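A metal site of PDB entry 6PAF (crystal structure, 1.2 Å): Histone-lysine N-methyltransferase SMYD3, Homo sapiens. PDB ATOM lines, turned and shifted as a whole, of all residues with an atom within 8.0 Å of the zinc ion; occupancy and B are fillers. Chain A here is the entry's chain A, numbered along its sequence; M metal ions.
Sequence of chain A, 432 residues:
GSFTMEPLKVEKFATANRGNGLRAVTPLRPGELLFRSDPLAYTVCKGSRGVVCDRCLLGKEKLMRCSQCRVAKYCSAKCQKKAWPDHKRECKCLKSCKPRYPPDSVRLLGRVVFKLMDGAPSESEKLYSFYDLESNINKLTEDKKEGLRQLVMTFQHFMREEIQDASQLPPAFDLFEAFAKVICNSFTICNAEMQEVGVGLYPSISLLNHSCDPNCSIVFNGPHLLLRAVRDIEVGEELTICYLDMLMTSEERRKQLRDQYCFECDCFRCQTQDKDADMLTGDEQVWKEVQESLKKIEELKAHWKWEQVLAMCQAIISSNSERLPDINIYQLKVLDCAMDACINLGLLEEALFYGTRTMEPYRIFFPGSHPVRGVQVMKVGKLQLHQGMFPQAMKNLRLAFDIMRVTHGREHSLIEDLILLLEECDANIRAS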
ATOM      1  N   VAL A  52       8.111  -6.404   0.798  1.00  0.00           N
ATOM      2  CA  VAL A  52       8.950  -5.234   0.619  1.00  0.00           C
ATOM      3  C   VAL A  52       9.191  -5.022  -0.864  1.00  0.00           C
ATOM      4  O   VAL A  52       9.131  -5.938  -1.678  1.00  0.00           O
ATOM      5  CB  VAL A  52      10.293  -5.316   1.372  1.00  0.00           C
ATOM      6  CG1 VAL A  52      10.046  -5.494   2.879  1.00  0.00           C
ATOM      7  CG2 VAL A  52      11.151  -6.426   0.838  1.00  0.00           C
ATOM      8  N   CYS A  53       9.553  -3.783  -1.182  1.00  0.00           N
ATOM      9  CA  CYS A  53       9.887  -3.428  -2.553  1.00  0.00           C
ATOM     10  C   CYS A  53      11.102  -4.209  -3.061  1.00  0.00           C
ATOM     11  O   CYS A  53      12.157  -4.226  -2.416  1.00  0.00           O
ATOM     12  CB  CYS A  53      10.181  -1.924  -2.614  1.00  0.00           C
ATOM     13  SG  CYS A  53      10.646  -1.306  -4.315  1.00  0.00           S
ATOM     14  N   ASP A  54      10.970  -4.828  -4.248  1.00  0.00           N
ATOM     15  CA  ASP A  54      12.095  -5.553  -4.858  1.00  0.00           C
ATOM     16  C   ASP A  54      13.317  -4.674  -5.003  1.00  0.00           C
ATOM     17  O   ASP A  54      14.440  -5.160  -4.911  1.00  0.00           O
ATOM     18  CB  ASP A  54      11.739  -5.936  -6.289  1.00  0.00           C
ATOM     19  CG  ASP A  54      11.261  -7.344  -6.431  1.00  0.00           C
ATOM     20  OD1 ASP A  54      10.345  -7.761  -5.696  1.00  0.00           O
ATOM     21  OD2 ASP A  54      11.791  -8.041  -7.309  1.00  0.00           O
ATOM     22  N   ARG A  55      13.116  -3.384  -5.280  1.00  0.00           N
ATOM     23  CA  ARG A  55      14.248  -2.513  -5.537  1.00  0.00           C
ATOM     24  C   ARG A  55      14.800  -1.937  -4.235  1.00  0.00           C
ATOM     25  O   ARG A  55      15.944  -2.203  -3.883  1.00  0.00           O
ATOM     26  CB  ARG A  55      13.877  -1.376  -6.526  1.00  0.00           C
ATOM     27  CG  ARG A  55      15.085  -0.539  -6.840  1.00  0.00           C
ATOM     28  CD  ARG A  55      14.861   0.399  -7.999  1.00  0.00           C
ATOM     29  NE  ARG A  55      15.948   1.378  -8.073  1.00  0.00           N
ATOM     30  CZ  ARG A  55      16.004   2.464  -7.322  1.00  0.00           C
ATOM     31  NH1 ARG A  55      15.028   2.721  -6.460  1.00  0.00           N
ATOM     32  NH2 ARG A  55      17.033   3.299  -7.426  1.00  0.00           N
ATOM     33  N   CYS A  56      14.013  -1.160  -3.495  1.00  0.00           N
ATOM     34  CA  CYS A  56      14.595  -0.442  -2.370  1.00  0.00           C
ATOM     35  C   CYS A  56      14.489  -1.221  -1.066  1.00  0.00           C
ATOM     36  O   CYS A  56      15.079  -0.768  -0.090  1.00  0.00           O
ATOM     37  CB  CYS A  56      13.985   0.950  -2.202  1.00  0.00           C
ATOM     38  SG  CYS A  56      12.222   0.933  -1.798  1.00  0.00           S
ATOM     39  N   LEU A  57      13.771  -2.355  -1.044  1.00  0.00           N
ATOM     40  CA  LEU A  57      13.699  -3.238   0.134  1.00  0.00           C
ATOM     41  C   LEU A  57      12.980  -2.586   1.317  1.00  0.00           C
ATOM     42  O   LEU A  57      13.178  -2.983   2.474  1.00  0.00           O
ATOM     43  CB  LEU A  57      15.069  -3.853   0.534  1.00  0.00           C
ATOM     44  CG  LEU A  57      15.800  -4.572  -0.611  1.00  0.00           C
ATOM     45  CD1 LEU A  57      17.163  -5.026  -0.094  1.00  0.00           C
ATOM     46  CD2 LEU A  57      15.003  -5.763  -1.135  1.00  0.00           C
ATOM     47  N   LEU A  58      12.125  -1.595   1.059  1.00  0.00           N
ATOM     48  CA  LEU A  58      11.308  -0.983   2.092  1.00  0.00           C
ATOM     49  C   LEU A  58       9.924  -1.604   2.032  1.00  0.00           C
ATOM     50  O   LEU A  58       9.415  -1.894   0.944  1.00  0.00           O
ATOM     51  CB  LEU A  58      11.173   0.528   1.847  1.00  0.00           C
ATOM     52  CG  LEU A  58      12.517   1.276   1.847  1.00  0.00           C
ATOM     53  CD1 LEU A  58      12.279   2.779   1.669  1.00  0.00           C
ATOM     54  CD2 LEU A  58      13.315   0.997   3.139  1.00  0.00           C
ATOM     55  N   GLY A  59       9.305  -1.772   3.205  1.00  0.00           N
ATOM     56  CA  GLY A  59       7.934  -2.245   3.240  1.00  0.00           C
ATOM     57  C   GLY A  59       6.952  -1.130   2.929  1.00  0.00           C
ATOM     58  O   GLY A  59       7.217   0.054   3.154  1.00  0.00           O
ATOM     59  N   LYS A  60       5.815  -1.514   2.365  1.00  0.00           N
ATOM     60  CA  LYS A  60       4.769  -0.537   2.046  1.00  0.00           C
ATOM     61  C   LYS A  60       3.391  -1.036   2.487  1.00  0.00           C
ATOM     62  O   LYS A  60       3.023  -2.176   2.216  1.00  0.00           O
ATOM     63  CB  LYS A  60       4.762  -0.227   0.551  1.00  0.00           C
ATOM     64  N   LEU A  63       1.935  -2.794  -2.459  1.00  0.00           N
ATOM     65  CA  LEU A  63       2.962  -2.854  -3.497  1.00  0.00           C
ATOM     66  C   LEU A  63       2.318  -3.022  -4.868  1.00  0.00           C
ATOM     67  O   LEU A  63       1.282  -3.666  -5.013  1.00  0.00           O
ATOM     68  CB  LEU A  63       3.933  -4.020  -3.256  1.00  0.00           C
ATOM     69  CG  LEU A  63       4.776  -4.037  -1.979  1.00  0.00           C
ATOM     70  CD1 LEU A  63       5.649  -5.255  -1.994  1.00  0.00           C
ATOM     71  CD2 LEU A  63       5.623  -2.784  -1.888  1.00  0.00           C
ATOM     72  N   LYS A  73       7.683  -6.976  -7.175  1.00  0.00           N
ATOM     73  CA  LYS A  73       6.733  -6.042  -6.608  1.00  0.00           C
ATOM     74  C   LYS A  73       7.480  -4.812  -6.100  1.00  0.00           C
ATOM     75  O   LYS A  73       8.605  -4.897  -5.614  1.00  0.00           O
ATOM     76  CB  LYS A  73       5.865  -6.676  -5.510  1.00  0.00           C
ATOM     77  CG  LYS A  73       4.798  -7.685  -6.025  1.00  0.00           C
ATOM     78  CD  LYS A  73       3.866  -8.101  -4.872  1.00  0.00           C
ATOM     79  CE  LYS A  73       2.720  -9.000  -5.302  1.00  0.00           C
ATOM     80  NZ  LYS A  73       3.193 -10.307  -5.814  1.00  0.00           N
ATOM     81  N   TYR A  74       6.821  -3.657  -6.208  1.00  0.00           N
ATOM     82  CA  TYR A  74       7.523  -2.405  -6.019  1.00  0.00           C
ATOM     83  C   TYR A  74       6.702  -1.421  -5.186  1.00  0.00           C
ATOM     84  O   TYR A  74       5.473  -1.441  -5.214  1.00  0.00           O
ATOM     85  CB  TYR A  74       7.869  -1.783  -7.368  1.00  0.00           C
ATOM     86  CG  TYR A  74       8.681  -2.684  -8.254  1.00  0.00           C
ATOM     87  CD1 TYR A  74      10.046  -2.850  -8.041  1.00  0.00           C
ATOM     88  CD2 TYR A  74       8.074  -3.388  -9.275  1.00  0.00           C
ATOM     89  CE1 TYR A  74      10.823  -3.663  -8.849  1.00  0.00           C
ATOM     90  CE2 TYR A  74       8.834  -4.205 -10.109  1.00  0.00           C
ATOM     91  CZ  TYR A  74      10.196  -4.346  -9.860  1.00  0.00           C
ATOM     92  OH  TYR A  74      10.956  -5.149 -10.693  1.00  0.00           O
ATOM     93  N   CYS A  75       7.417  -0.531  -4.509  1.00  0.00           N
ATOM     94  CA  CYS A  75       6.795   0.495  -3.694  1.00  0.00           C
ATOM     95  C   CYS A  75       6.262   1.694  -4.482  1.00  0.00           C
ATOM     96  O   CYS A  75       5.396   2.415  -3.962  1.00  0.00           O
ATOM     97  CB  CYS A  75       7.815   1.012  -2.702  1.00  0.00           C
ATOM     98  SG  CYS A  75       9.098   2.148  -3.311  1.00  0.00           S
ATOM     99  N   SER A  76       6.762   1.921  -5.696  1.00  0.00           N
ATOM    100  CA  SER A  76       6.488   3.146  -6.437  1.00  0.00           C
ATOM    101  C   SER A  76       6.779   2.879  -7.903  1.00  0.00           C
ATOM    102  O   SER A  76       7.509   1.959  -8.258  1.00  0.00           O
ATOM    103  CB  SER A  76       7.401   4.278  -5.944  1.00  0.00           C
ATOM    104  OG  SER A  76       8.775   3.877  -6.069  1.00  0.00           O
ATOM    105  N   ALA A  77       6.205   3.736  -8.753  1.00  0.00           N
ATOM    106  CA  ALA A  77       6.553   3.668 -10.166  1.00  0.00           C
ATOM    107  C   ALA A  77       8.038   3.907 -10.356  1.00  0.00           C
ATOM    108  O   ALA A  77       8.667   3.275 -11.216  1.00  0.00           O
ATOM    109  CB  ALA A  77       5.707   4.687 -10.934  1.00  0.00           C
ATOM    110  N   LYS A  78       8.639   4.761  -9.517  1.00  0.00           N
ATOM    111  CA  LYS A  78      10.052   5.068  -9.635  1.00  0.00           C
ATOM    112  C   LYS A  78      10.864   3.794  -9.457  1.00  0.00           C
ATOM    113  O   LYS A  78      11.759   3.486 -10.252  1.00  0.00           O
ATOM    114  CB  LYS A  78      10.464   6.135  -8.604  1.00  0.00           C
ATOM    115  CG  LYS A  78      11.980   6.370  -8.592  1.00  0.00           C
ATOM    116  CD  LYS A  78      12.389   7.431  -7.574  1.00  0.00           C
ATOM    117  CE  LYS A  78      13.897   7.579  -7.535  1.00  0.00           C
ATOM    118  N   CYS A  79      10.564   3.038  -8.399  1.00  0.00           N
ATOM    119  CA  CYS A  79      11.299   1.806  -8.176  1.00  0.00           C
ATOM    120  C   CYS A  79      11.014   0.773  -9.251  1.00  0.00           C
ATOM    121  O   CYS A  79      11.931   0.077  -9.676  1.00  0.00           O
ATOM    122  CB  CYS A  79      10.950   1.233  -6.818  1.00  0.00           C
ATOM    123  SG  CYS A  79      11.961   2.021  -5.497  1.00  0.00           S
ATOM    124  N   GLN A  80       9.741   0.639  -9.680  1.00  0.00           N
ATOM    125  CA  GLN A  80       9.456  -0.377 -10.707  1.00  0.00           C
ATOM    126  C   GLN A  80      10.192  -0.055 -11.987  1.00  0.00           C
ATOM    127  O   GLN A  80      10.794  -0.947 -12.614  1.00  0.00           O
ATOM    128  CB  GLN A  80       7.962  -0.505 -10.982  1.00  0.00           C
ATOM    129  CG  GLN A  80       7.652  -1.506 -12.099  1.00  0.00           C
ATOM    130  CD  GLN A  80       6.183  -1.789 -12.244  1.00  0.00           C
ATOM    131  OE1 GLN A  80       5.381  -1.345 -11.415  1.00  0.00           O
ATOM    132  NE2 GLN A  80       5.813  -2.509 -13.288  1.00  0.00           N
HETATM  133 ZN    ZN M   1      11.075   1.021  -3.670  1.00  0.00          ZN
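Four residues have an atom within 4 Å of the zinc ion: Cys 53, Cys 56, Cys 75 and Cys 79.
The zinc ion is bound by the side-chain sulfur (SG) of Cys 56 (2.2 Å), the side-chain sulfur (SG) of Cys 79 (2.3 Å), the side-chain sulfur (SG) of Cys 75 (2.3 Å) and the side-chain sulfur (SG) of Cys 53 (2.5 Å). The zinc ion has four donor atoms within binding distance.
N of Cys 79 sits at hydrogen-bond distance from OG of Ser 76 (3.1 Å). The side-chain sulfur (SG) of Cys 79 lies close to the guanidinium group (NH1) of Arg 55, 3.3 Å away. The side-chain sulfur (SG) of Cys 75 lies close to the side-chain hydroxyl (OG) of Ser 76 (3.3 Å). The side-chain sulfur (SG) of Cys 53 lies close to the backbone NH (N) of Arg 55, 3.4 Å away. The backbone NH (N) of Cys 53 lies within hydrogen-bond range of the backbone carbonyl oxygen (O) of Leu 58 (2.8 Å).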
